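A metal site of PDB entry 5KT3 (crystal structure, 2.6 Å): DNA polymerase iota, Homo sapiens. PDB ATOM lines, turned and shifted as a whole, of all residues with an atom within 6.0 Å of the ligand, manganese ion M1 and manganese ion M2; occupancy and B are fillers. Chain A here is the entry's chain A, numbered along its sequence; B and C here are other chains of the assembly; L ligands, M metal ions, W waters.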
ATOM      1  N   ASP A  34      -5.376   7.917 -19.032  1.00  0.00           N
ATOM      2  CA  ASP A  34      -4.740   9.212 -19.242  1.00  0.00           C
ATOM      3  C   ASP A  34      -5.353  10.191 -18.269  1.00  0.00           C
ATOM      4  O   ASP A  34      -6.575  10.224 -18.105  1.00  0.00           O
ATOM      5  CB  ASP A  34      -4.941   9.721 -20.683  1.00  0.00           C
ATOM      6  CG  ASP A  34      -4.307  11.072 -20.917  1.00  0.00           C
ATOM      7  OD1 ASP A  34      -3.566  11.208 -21.892  1.00  0.00           O
ATOM      8  OD2 ASP A  34      -4.571  12.025 -20.145  1.00  0.00           O
ATOM      9  N   LEU A  35      -4.525  11.038 -17.653  1.00  0.00           N
ATOM     10  CA  LEU A  35      -5.029  11.868 -16.582  1.00  0.00           C
ATOM     11  C   LEU A  35      -5.571  13.192 -17.108  1.00  0.00           C
ATOM     12  O   LEU A  35      -5.067  13.736 -18.095  1.00  0.00           O
ATOM     13  CB  LEU A  35      -3.935  12.127 -15.559  1.00  0.00           C
ATOM     14  CG  LEU A  35      -3.521  10.841 -14.863  1.00  0.00           C
ATOM     15  CD1 LEU A  35      -2.417  11.119 -13.889  1.00  0.00           C
ATOM     16  CD2 LEU A  35      -4.698  10.286 -14.125  1.00  0.00           C
ATOM     17  N   ASP A  36      -6.609  13.693 -16.452  1.00  0.00           N
ATOM     18  CA  ASP A  36      -7.185  14.989 -16.786  1.00  0.00           C
ATOM     19  C   ASP A  36      -6.227  16.118 -16.414  1.00  0.00           C
ATOM     20  O   ASP A  36      -5.814  16.228 -15.246  1.00  0.00           O
ATOM     21  CB  ASP A  36      -8.505  15.200 -16.056  1.00  0.00           C
ATOM     22  CG  ASP A  36      -9.516  14.100 -16.309  1.00  0.00           C
ATOM     23  OD1 ASP A  36      -9.523  13.518 -17.416  1.00  0.00           O
ATOM     24  OD2 ASP A  36     -10.308  13.838 -15.393  1.00  0.00           O
ATOM     25  N   CYS A  37      -5.920  16.980 -17.394  1.00  0.00           N
ATOM     26  CA  CYS A  37      -5.079  18.171 -17.222  1.00  0.00           C
ATOM     27  C   CYS A  37      -4.033  17.991 -16.136  1.00  0.00           C
ATOM     28  O   CYS A  37      -3.971  18.776 -15.172  1.00  0.00           O
ATOM     29  CB  CYS A  37      -5.951  19.402 -16.955  1.00  0.00           C
ATOM     30  SG  CYS A  37      -7.085  19.244 -15.538  1.00  0.00           S
ATOM     31  N   PHE A  38      -3.194  16.963 -16.294  1.00  0.00           N
ATOM     32  CA  PHE A  38      -2.435  16.390 -15.186  1.00  0.00           C
ATOM     33  C   PHE A  38      -1.779  17.457 -14.324  1.00  0.00           C
ATOM     34  O   PHE A  38      -2.056  17.553 -13.115  1.00  0.00           O
ATOM     35  CB  PHE A  38      -1.383  15.411 -15.740  1.00  0.00           C
ATOM     36  CG  PHE A  38      -0.554  14.756 -14.684  1.00  0.00           C
ATOM     37  CD1 PHE A  38      -1.135  14.279 -13.513  1.00  0.00           C
ATOM     38  CD2 PHE A  38       0.809  14.622 -14.853  1.00  0.00           C
ATOM     39  CE1 PHE A  38      -0.360  13.671 -12.523  1.00  0.00           C
ATOM     40  CE2 PHE A  38       1.600  14.020 -13.878  1.00  0.00           C
ATOM     41  CZ  PHE A  38       1.011  13.544 -12.702  1.00  0.00           C
ATOM     42  N   TYR A  39      -0.874  18.244 -14.908  1.00  0.00           N
ATOM     43  CA  TYR A  39      -0.114  19.204 -14.090  1.00  0.00           C
ATOM     44  C   TYR A  39      -1.077  20.143 -13.372  1.00  0.00           C
ATOM     45  O   TYR A  39      -1.003  20.325 -12.143  1.00  0.00           O
ATOM     46  CB  TYR A  39       0.854  20.016 -14.956  1.00  0.00           C
ATOM     47  CG  TYR A  39       2.076  19.284 -15.456  1.00  0.00           C
ATOM     48  CD1 TYR A  39       2.249  17.911 -15.252  1.00  0.00           C
ATOM     49  CD2 TYR A  39       3.081  19.979 -16.136  1.00  0.00           C
ATOM     50  CE1 TYR A  39       3.380  17.247 -15.732  1.00  0.00           C
ATOM     51  CE2 TYR A  39       4.219  19.341 -16.595  1.00  0.00           C
ATOM     52  CZ  TYR A  39       4.367  17.983 -16.398  1.00  0.00           C
ATOM     53  OH  TYR A  39       5.488  17.359 -16.870  1.00  0.00           O
ATOM     54  N   ALA A  40      -2.000  20.742 -14.129  1.00  0.00           N
ATOM     55  CA  ALA A  40      -3.019  21.589 -13.548  1.00  0.00           C
ATOM     56  C   ALA A  40      -3.757  20.868 -12.430  1.00  0.00           C
ATOM     57  O   ALA A  40      -4.021  21.457 -11.383  1.00  0.00           O
ATOM     58  CB  ALA A  40      -3.985  22.057 -14.626  1.00  0.00           C
ATOM     59  N   GLN A  59       5.664  26.995 -18.251  1.00  0.00           N
ATOM     60  CA  GLN A  59       7.075  26.637 -18.238  1.00  0.00           C
ATOM     61  C   GLN A  59       7.766  27.577 -19.217  1.00  0.00           C
ATOM     62  O   GLN A  59       7.615  27.439 -20.433  1.00  0.00           O
ATOM     63  CB  GLN A  59       7.271  25.172 -18.635  1.00  0.00           C
ATOM     64  CG  GLN A  59       6.658  24.159 -17.677  1.00  0.00           C
ATOM     65  CD  GLN A  59       6.911  22.727 -18.111  1.00  0.00           C
ATOM     66  OE1 GLN A  59       6.938  22.436 -19.309  1.00  0.00           O
ATOM     67  NE2 GLN A  59       7.133  21.835 -17.149  1.00  0.00           N
ATOM     68  N   VAL A  64       1.738  24.901 -20.657  1.00  0.00           N
ATOM     69  CA  VAL A  64       1.958  23.543 -21.135  1.00  0.00           C
ATOM     70  C   VAL A  64       0.680  22.732 -20.988  1.00  0.00           C
ATOM     71  O   VAL A  64       0.394  21.855 -21.818  1.00  0.00           O
ATOM     72  CB  VAL A  64       3.192  22.953 -20.416  1.00  0.00           C
ATOM     73  CG1 VAL A  64       2.872  22.441 -19.014  1.00  0.00           C
ATOM     74  CG2 VAL A  64       3.831  21.884 -21.273  1.00  0.00           C
ATOM     75  N   THR A  65      -0.153  23.061 -20.003  1.00  0.00           N
ATOM     76  CA  THR A  65      -1.519  22.563 -19.942  1.00  0.00           C
ATOM     77  C   THR A  65      -2.348  23.607 -19.197  1.00  0.00           C
ATOM     78  O   THR A  65      -1.825  24.556 -18.613  1.00  0.00           O
ATOM     79  CB  THR A  65      -1.593  21.188 -19.276  1.00  0.00           C
ATOM     80  OG1 THR A  65      -2.942  20.684 -19.325  1.00  0.00           O
ATOM     81  CG2 THR A  65      -1.143  21.259 -17.833  1.00  0.00           C
ATOM     82  N   CYS A  66      -3.673  23.407 -19.237  1.00  0.00           N
ATOM     83  CA  CYS A  66      -4.584  24.250 -18.475  1.00  0.00           C
ATOM     84  C   CYS A  66      -5.775  23.398 -18.047  1.00  0.00           C
ATOM     85  O   CYS A  66      -6.048  22.362 -18.657  1.00  0.00           O
ATOM     86  CB  CYS A  66      -5.069  25.440 -19.293  1.00  0.00           C
ATOM     87  SG  CYS A  66      -5.839  24.924 -20.811  1.00  0.00           S
ATOM     88  N   TYR A  68      -9.930  22.690 -17.100  1.00  0.00           N
ATOM     89  CA  TYR A  68     -11.009  22.687 -18.074  1.00  0.00           C
ATOM     90  C   TYR A  68     -11.809  23.991 -18.072  1.00  0.00           C
ATOM     91  O   TYR A  68     -12.366  24.347 -19.119  1.00  0.00           O
ATOM     92  CB  TYR A  68     -11.887  21.456 -17.856  1.00  0.00           C
ATOM     93  CG  TYR A  68     -11.279  20.265 -18.559  1.00  0.00           C
ATOM     94  CD1 TYR A  68     -10.190  19.576 -18.007  1.00  0.00           C
ATOM     95  CD2 TYR A  68     -11.737  19.851 -19.808  1.00  0.00           C
ATOM     96  CE1 TYR A  68      -9.604  18.489 -18.667  1.00  0.00           C
ATOM     97  CE2 TYR A  68     -11.156  18.760 -20.475  1.00  0.00           C
ATOM     98  CZ  TYR A  68     -10.095  18.083 -19.896  1.00  0.00           C
ATOM     99  OH  TYR A  68      -9.501  17.024 -20.553  1.00  0.00           O
ATOM    100  N   ARG A  71     -10.026  25.879 -20.614  1.00  0.00           N
ATOM    101  CA  ARG A  71     -10.315  25.428 -21.963  1.00  0.00           C
ATOM    102  C   ARG A  71     -11.684  25.914 -22.433  1.00  0.00           C
ATOM    103  O   ARG A  71     -11.867  26.163 -23.628  1.00  0.00           O
ATOM    104  CB  ARG A  71     -10.229  23.902 -22.047  1.00  0.00           C
ATOM    105  CG  ARG A  71      -8.811  23.379 -21.919  1.00  0.00           C
ATOM    106  CD  ARG A  71      -8.738  21.862 -21.869  1.00  0.00           C
ATOM    107  NE  ARG A  71      -7.623  21.433 -21.032  1.00  0.00           N
ATOM    108  CZ  ARG A  71      -6.993  20.260 -21.129  1.00  0.00           C
ATOM    109  NH1 ARG A  71      -7.338  19.376 -22.054  1.00  0.00           N
ATOM    110  NH2 ARG A  71      -6.009  19.990 -20.293  1.00  0.00           N
ATOM    111  N   LYS A  77      -3.902  23.544 -24.880  1.00  0.00           N
ATOM    112  CA  LYS A  77      -2.641  22.995 -24.428  1.00  0.00           C
ATOM    113  C   LYS A  77      -1.507  23.430 -25.352  1.00  0.00           C
ATOM    114  O   LYS A  77      -1.668  23.466 -26.570  1.00  0.00           O
ATOM    115  CB  LYS A  77      -2.714  21.468 -24.361  1.00  0.00           C
ATOM    116  CG  LYS A  77      -3.718  20.962 -23.312  1.00  0.00           C
ATOM    117  CD  LYS A  77      -3.950  19.451 -23.397  1.00  0.00           C
ATOM    118  CE  LYS A  77      -4.530  19.038 -24.713  1.00  0.00           C
ATOM    119  NZ  LYS A  77      -5.438  17.846 -24.559  1.00  0.00           N
ATOM    120  N   LEU A  78      -0.364  23.768 -24.754  1.00  0.00           N
ATOM    121  CA  LEU A  78       0.847  24.161 -25.474  1.00  0.00           C
ATOM    122  C   LEU A  78       0.663  25.468 -26.229  1.00  0.00           C
ATOM    123  O   LEU A  78       1.242  25.665 -27.298  1.00  0.00           O
ATOM    124  CB  LEU A  78       1.311  23.035 -26.403  1.00  0.00           C
ATOM    125  CG  LEU A  78       1.479  21.674 -25.714  1.00  0.00           C
ATOM    126  CD1 LEU A  78       1.710  20.561 -26.722  1.00  0.00           C
ATOM    127  CD2 LEU A  78       2.605  21.722 -24.678  1.00  0.00           C
ATOM    128  N   LEU A 123       3.618   5.630 -20.231  1.00  0.00           N
ATOM    129  CA  LEU A 123       3.909   6.426 -21.411  1.00  0.00           C
ATOM    130  C   LEU A 123       3.871   7.884 -20.984  1.00  0.00           C
ATOM    131  O   LEU A 123       2.795   8.413 -20.680  1.00  0.00           O
ATOM    132  CB  LEU A 123       2.922   6.148 -22.546  1.00  0.00           C
ATOM    133  CG  LEU A 123       3.251   6.834 -23.878  1.00  0.00           C
ATOM    134  CD1 LEU A 123       4.646   6.425 -24.408  1.00  0.00           C
ATOM    135  CD2 LEU A 123       2.153   6.561 -24.903  1.00  0.00           C
ATOM    136  N   PHE A 125       4.321  10.948 -18.309  1.00  0.00           N
ATOM    137  CA  PHE A 125       4.032  10.997 -16.884  1.00  0.00           C
ATOM    138  C   PHE A 125       2.599  10.653 -16.536  1.00  0.00           C
ATOM    139  O   PHE A 125       2.332  10.372 -15.367  1.00  0.00           O
ATOM    140  CB  PHE A 125       4.309  12.394 -16.303  1.00  0.00           C
ATOM    141  CG  PHE A 125       5.748  12.656 -15.976  1.00  0.00           C
ATOM    142  CD1 PHE A 125       6.098  13.775 -15.209  1.00  0.00           C
ATOM    143  CD2 PHE A 125       6.748  11.813 -16.430  1.00  0.00           C
ATOM    144  CE1 PHE A 125       7.424  14.038 -14.912  1.00  0.00           C
ATOM    145  CE2 PHE A 125       8.080  12.072 -16.121  1.00  0.00           C
ATOM    146  CZ  PHE A 125       8.418  13.190 -15.373  1.00  0.00           C
ATOM    147  N   ASP A 126       1.660  10.723 -17.479  1.00  0.00           N
ATOM    148  CA  ASP A 126       0.248  10.679 -17.088  1.00  0.00           C
ATOM    149  C   ASP A 126      -0.543   9.594 -17.793  1.00  0.00           C
ATOM    150  O   ASP A 126      -1.779   9.604 -17.703  1.00  0.00           O
ATOM    151  CB  ASP A 126      -0.405  12.048 -17.302  1.00  0.00           C
ATOM    152  CG  ASP A 126      -1.005  12.216 -18.688  1.00  0.00           C
ATOM    153  OD1 ASP A 126      -0.375  11.745 -19.663  1.00  0.00           O
ATOM    154  OD2 ASP A 126      -2.108  12.800 -18.807  1.00  0.00           O
ATOM    155  N   GLU A 127       0.109   8.637 -18.450  1.00  0.00           N
ATOM    156  CA  GLU A 127      -0.576   7.574 -19.163  1.00  0.00           C
ATOM    157  C   GLU A 127      -0.019   6.223 -18.760  1.00  0.00           C
ATOM    158  O   GLU A 127       1.194   6.061 -18.593  1.00  0.00           O
ATOM    159  CB  GLU A 127      -0.462   7.738 -20.682  1.00  0.00           C
ATOM    160  CG  GLU A 127      -1.305   8.878 -21.208  1.00  0.00           C
ATOM    161  CD  GLU A 127      -1.026   9.186 -22.664  1.00  0.00           C
ATOM    162  OE1 GLU A 127      -0.932   8.238 -23.486  1.00  0.00           O
ATOM    163  OE2 GLU A 127      -0.898  10.393 -22.978  1.00  0.00           O
ATOM    164  N   LYS A 207      -5.661   3.368 -26.601  1.00  0.00           N
ATOM    165  CA  LYS A 207      -5.225   4.752 -26.464  1.00  0.00           C
ATOM    166  C   LYS A 207      -6.051   5.700 -27.328  1.00  0.00           C
ATOM    167  O   LYS A 207      -6.272   6.853 -26.934  1.00  0.00           O
ATOM    168  CB  LYS A 207      -3.742   4.901 -26.796  1.00  0.00           C
ATOM    169  CG  LYS A 207      -3.205   6.322 -26.603  1.00  0.00           C
ATOM    170  CD  LYS A 207      -1.797   6.466 -27.178  1.00  0.00           C
ATOM    171  CE  LYS A 207      -0.994   7.523 -26.463  1.00  0.00           C
ATOM    172  NZ  LYS A 207      -1.571   8.859 -26.596  1.00  0.00           N
ATOM    173  N   LYS A 214     -14.171  13.060 -22.774  1.00  0.00           N
ATOM    174  CA  LYS A 214     -13.349  13.752 -21.812  1.00  0.00           C
ATOM    175  C   LYS A 214     -14.128  14.900 -21.180  1.00  0.00           C
ATOM    176  O   LYS A 214     -14.964  15.504 -21.833  1.00  0.00           O
ATOM    177  CB  LYS A 214     -12.106  14.330 -22.487  1.00  0.00           C
ATOM    178  CG  LYS A 214     -11.151  13.309 -23.010  1.00  0.00           C
ATOM    179  CD  LYS A 214     -10.195  13.975 -23.979  1.00  0.00           C
ATOM    180  CE  LYS A 214      -9.249  14.893 -23.273  1.00  0.00           C
ATOM    181  NZ  LYS A 214      -8.369  15.555 -24.268  1.00  0.00           N
ATOM    182  N   PRO A 215     -13.801  15.240 -19.924  1.00  0.00           N
ATOM    183  CA  PRO A 215     -12.826  14.507 -19.109  1.00  0.00           C
ATOM    184  C   PRO A 215     -13.468  13.525 -18.152  1.00  0.00           C
ATOM    185  O   PRO A 215     -14.697  13.434 -18.111  1.00  0.00           O
ATOM    186  CB  PRO A 215     -12.124  15.625 -18.348  1.00  0.00           C
ATOM    187  CG  PRO A 215     -13.200  16.635 -18.144  1.00  0.00           C
ATOM    188  CD  PRO A 215     -14.089  16.564 -19.370  1.00  0.00           C
ATOM    189  P    DC B   7       1.440  10.982 -27.664  1.00  0.00           P
ATOM    190  OP1  DC B   7       0.056  10.497 -27.498  1.00  0.00           O
ATOM    191  OP2  DC B   7       1.830  11.969 -28.709  1.00  0.00           O
ATOM    192  O5'  DC B   7       1.837  11.554 -26.237  1.00  0.00           O
ATOM    193  C5'  DC B   7       1.334  10.908 -25.091  1.00  0.00           C
ATOM    194  C4'  DC B   7       1.816  11.605 -23.846  1.00  0.00           C
ATOM    195  O4'  DC B   7       3.243  11.696 -23.893  1.00  0.00           O
ATOM    196  C3'  DC B   7       1.363  13.040 -23.710  1.00  0.00           C
ATOM    197  O3'  DC B   7       0.061  13.081 -23.146  1.00  0.00           O
ATOM    198  C2'  DC B   7       2.394  13.578 -22.738  1.00  0.00           C
ATOM    199  C1'  DC B   7       3.661  12.811 -23.130  1.00  0.00           C
ATOM    200  N1   DC B   7       4.577  13.624 -23.943  1.00  0.00           N
ATOM    201  C2   DC B   7       5.415  14.539 -23.297  1.00  0.00           C
ATOM    202  O2   DC B   7       5.371  14.630 -22.073  1.00  0.00           O
ATOM    203  N3   DC B   7       6.249  15.286 -24.044  1.00  0.00           N
ATOM    204  C4   DC B   7       6.263  15.157 -25.363  1.00  0.00           C
ATOM    205  N4   DC B   7       7.109  15.916 -26.056  1.00  0.00           N
ATOM    206  C5   DC B   7       5.417  14.234 -26.041  1.00  0.00           C
ATOM    207  C6   DC B   7       4.596  13.498 -25.296  1.00  0.00           C
ATOM    208  P    DG C   3      10.461  28.048 -24.334  1.00  0.00           P
ATOM    209  OP1  DG C   3       9.228  28.798 -23.998  1.00  0.00           O
ATOM    210  OP2  DG C   3      11.780  28.735 -24.365  1.00  0.00           O
ATOM    211  O5'  DG C   3      10.663  26.818 -23.359  1.00  0.00           O
ATOM    212  C5'  DG C   3       9.689  25.806 -23.284  1.00  0.00           C
ATOM    213  C4'  DG C   3       9.592  25.329 -21.858  1.00  0.00           C
ATOM    214  O4'  DG C   3       8.539  24.340 -21.725  1.00  0.00           O
ATOM    215  C3'  DG C   3      10.840  24.662 -21.326  1.00  0.00           C
ATOM    216  O3'  DG C   3      10.844  24.820 -19.927  1.00  0.00           O
ATOM    217  C2'  DG C   3      10.613  23.199 -21.738  1.00  0.00           C
ATOM    218  C1'  DG C   3       9.107  23.055 -21.507  1.00  0.00           C
ATOM    219  N9   DG C   3       8.401  22.135 -22.408  1.00  0.00           N
ATOM    220  C8   DG C   3       7.425  21.249 -22.046  1.00  0.00           C
ATOM    221  N7   DG C   3       6.922  20.585 -23.038  1.00  0.00           N
ATOM    222  C5   DG C   3       7.611  21.067 -24.150  1.00  0.00           C
ATOM    223  C6   DG C   3       7.492  20.715 -25.511  1.00  0.00           C
ATOM    224  O6   DG C   3       6.729  19.872 -26.020  1.00  0.00           O
ATOM    225  N1   DG C   3       8.361  21.437 -26.310  1.00  0.00           N
ATOM    226  C2   DG C   3       9.243  22.390 -25.841  1.00  0.00           C
ATOM    227  N2   DG C   3      10.011  22.987 -26.762  1.00  0.00           N
ATOM    228  N3   DG C   3       9.370  22.728 -24.562  1.00  0.00           N
ATOM    229  C4   DG C   3       8.520  22.025 -23.776  1.00  0.00           C
ATOM    230  P    DG C   4      12.164  24.524 -19.094  1.00  0.00           P
ATOM    231  OP1  DG C   4      12.220  25.375 -17.885  1.00  0.00           O
ATOM    232  OP2  DG C   4      13.241  24.509 -20.085  1.00  0.00           O
ATOM    233  O5'  DG C   4      11.937  23.024 -18.598  1.00  0.00           O
ATOM    234  C5'  DG C   4      10.894  22.722 -17.710  1.00  0.00           C
ATOM    235  C4'  DG C   4      10.732  21.238 -17.649  1.00  0.00           C
ATOM    236  O4'  DG C   4      10.123  20.780 -18.897  1.00  0.00           O
ATOM    237  C3'  DG C   4      12.055  20.471 -17.550  1.00  0.00           C
ATOM    238  O3'  DG C   4      11.959  19.467 -16.542  1.00  0.00           O
ATOM    239  C2'  DG C   4      12.216  19.868 -18.944  1.00  0.00           C
ATOM    240  C1'  DG C   4      10.762  19.611 -19.278  1.00  0.00           C
ATOM    241  N9   DG C   4      10.523  19.360 -20.679  1.00  0.00           N
ATOM    242  C8   DG C   4      11.232  19.852 -21.740  1.00  0.00           C
ATOM    243  N7   DG C   4      10.793  19.428 -22.895  1.00  0.00           N
ATOM    244  C5   DG C   4       9.741  18.578 -22.574  1.00  0.00           C
ATOM    245  C6   DG C   4       8.885  17.828 -23.411  1.00  0.00           C
ATOM    246  O6   DG C   4       8.882  17.759 -24.644  1.00  0.00           O
ATOM    247  N1   DG C   4       7.941  17.113 -22.662  1.00  0.00           N
ATOM    248  C2   DG C   4       7.852  17.126 -21.304  1.00  0.00           C
ATOM    249  N2   DG C   4       6.895  16.367 -20.759  1.00  0.00           N
ATOM    250  N3   DG C   4       8.655  17.816 -20.514  1.00  0.00           N
ATOM    251  C4   DG C   4       9.566  18.520 -21.216  1.00  0.00           C
HETATM  252  P1  LIG L   1      -5.766  16.062 -20.967  1.00  0.00           P
HETATM  253  O1  LIG L   1      -5.036  14.731 -20.997  1.00  0.00           O
HETATM  254  O2  LIG L   1      -6.187  16.540 -22.348  1.00  0.00           O
HETATM  255  O3  LIG L   1      -6.833  16.154 -19.909  1.00  0.00           O
HETATM  256  P2  LIG L   1      -3.204  16.847 -19.985  1.00  0.00           P
HETATM  257  O4  LIG L   1      -2.700  18.060 -19.273  1.00  0.00           O
HETATM  258  O5  LIG L   1      -3.154  15.561 -19.203  1.00  0.00           O
HETATM  259  O6  LIG L   1      -4.724  17.156 -20.402  1.00  0.00           O
HETATM  260  P3  LIG L   1      -1.459  15.346 -21.787  1.00  0.00           P
HETATM  261  O7  LIG L   1      -1.039  15.380 -23.241  1.00  0.00           O
HETATM  262  O8  LIG L   1      -2.289  14.213 -21.286  1.00  0.00           O
HETATM  263  N1  LIG L   1      -2.351  16.819 -21.505  1.00  0.00           N
HETATM  264  O9  LIG L   1      -0.052  15.450 -20.976  1.00  0.00           O
HETATM  265  C1  LIG L   1       0.041  15.226 -19.585  1.00  0.00           C
HETATM  266  C2  LIG L   1       0.911  16.297 -18.902  1.00  0.00           C
HETATM  267  O10 LIG L   1       2.228  16.260 -19.423  1.00  0.00           O
HETATM  268  C3  LIG L   1       0.426  17.727 -19.114  1.00  0.00           C
HETATM  269  O11 LIG L   1      -0.477  18.146 -18.082  1.00  0.00           O
HETATM  270  C4  LIG L   1       1.689  18.546 -19.110  1.00  0.00           C
HETATM  271  C5  LIG L   1       2.773  17.569 -19.532  1.00  0.00           C
HETATM  272  N2  LIG L   1       3.161  17.748 -20.935  1.00  0.00           N
HETATM  273  C6  LIG L   1       4.270  18.554 -21.225  1.00  0.00           C
HETATM  274  N3  LIG L   1       4.662  18.738 -22.504  1.00  0.00           N
HETATM  275  C7  LIG L   1       4.010  18.127 -23.509  1.00  0.00           C
HETATM  276  C8  LIG L   1       2.912  17.320 -23.242  1.00  0.00           C
HETATM  277  C9  LIG L   1       2.508  17.135 -21.923  1.00  0.00           C
HETATM  278  O12 LIG L   1       4.895  19.109 -20.304  1.00  0.00           O
HETATM  279  N4  LIG L   1       4.447  18.333 -24.781  1.00  0.00           N
HETATM  280 MN    MN M   1      -3.734  13.757 -19.724  1.00  0.00          MN
HETATM  281 MN    MN M   2      -1.535  12.201 -21.857  1.00  0.00          MN
HETATM  282  O   HOH W   1      -4.428  13.956 -23.803  1.00  0.00           O
HETATM  283  O   HOH W   2       3.154  17.010 -27.173  1.00  0.00           O
HETATM  284  O   HOH W   3      -0.623  17.594 -24.680  1.00  0.00           O
HETATM  285  O   HOH W   4       6.935  18.739 -18.793  1.00  0.00           O
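OG1 of Thr 65 lies within hydrogen-bond range of O4 of the ligand (2.6 Å).
An oxygen (O2) of the ligand lies within salt-bridge range of the side-chain amino group of Lys 77.
The backbone NH (N) of Cys 37 lies within hydrogen-bond range of an oxygen (O3) of the ligand, 2.8 Å away.
An oxygen (O3) of the ligand sits at hydrogen-bond distance from the side-chain hydroxyl of Tyr 68 (2.9 Å).
O6 of DG 3 of chain C is in hydrogen-bond range of N4 of the ligand.
O2 of the ligand is in salt-bridge range of NZ of Lys 214.
The guanidinium group of Arg 71 is in salt-bridge range of an oxygen (O2) of the ligand (3.1 Å).
The backbone NH (N) of Tyr 39 is in hydrogen-bond range of an oxygen (O11) of the ligand (3.2 Å).
The backbone NH (N) of Phe 38 is in hydrogen-bond range of an oxygen (O4) of the ligand (3.2 Å).
The side-chain carboxylate of Glu 127 lies within salt-bridge range of the side-chain amino group of Lys 207 (3.2 Å).
O2 of DC 7 of chain B sits close to N2 of DG 4 of chain C, 2.7 Å away.
OP1 of DC 7 of chain B is in salt-bridge range of the side-chain amino group of Lys 207 (2.5 Å).
The guanidinium group of Arg 71 is in hydrogen-bond range of the side-chain hydroxyl of Thr 65, 3.3 Å away.
N9 of DG 3 of chain C lies close to the side-chain amide oxygen (OE1) of Gln 59 (3.4 Å).
The guanidinium group of Arg 71 lies within hydrogen-bond range of the backbone carbonyl oxygen of Cys 66 (2.9 Å).
An oxygen (O12) of the ligand lies close to N2 of DG 4 of chain C.
Asp 36 touches the ligand.
Val 64 touches the ligand.
Leu 78 touches the ligand.
17 residues have an atom within 4 Å of the ligand: Asp 34, Leu 35, Asp 36, Cys 37, Phe 38, Tyr 39, Val 64, Thr 65, Tyr 68, Arg 71, Lys 77, Leu 78, Asp 126, Lys 214, DC 7 of chain B, DG 3 of chain C and DG 4 of chain C.
Of the 25 residues printed, 3 come within 4 Å of manganese ion M1.
Four residues have an atom within 4 Å of manganese ion M2: Asp 34, Asp 126, Glu 127 and DC 7 of chain B.
The nearest printed residue that does not touch manganese ion M2 is Leu 35 (5.3 Å).
O5 of the ligand is bound to manganese ion M1 (2.0 Å).
Manganese ion M1 is bound by the side-chain carboxylate (OD2) of Asp 34.
O1 of the ligand is bound to manganese ion M1, at 2.1 Å.
Manganese ion M1 is bound by OD2 of Asp 126 (2.1 Å).
O of Leu 35 binds manganese ion M1, 2.1 Å away.
Manganese ion M1 is bound by O8 of the ligand (2.2 Å).
Manganese ion M2 is bound by OE2 of Glu 127 (2.2 Å), O8 of the ligand (2.2 Å), O3' of DC 7 of chain B (2.2 Å), OD1 of Asp 34 (2.3 Å) and OD1 of Asp 126 (2.5 Å).
Water W4 lies within hydrogen-bond range of an oxygen (O12) of the ligand (2.6 Å), N3 of DG 4 of chain C (2.6 Å) and the side-chain hydroxyl of Tyr 39 (2.8 Å).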
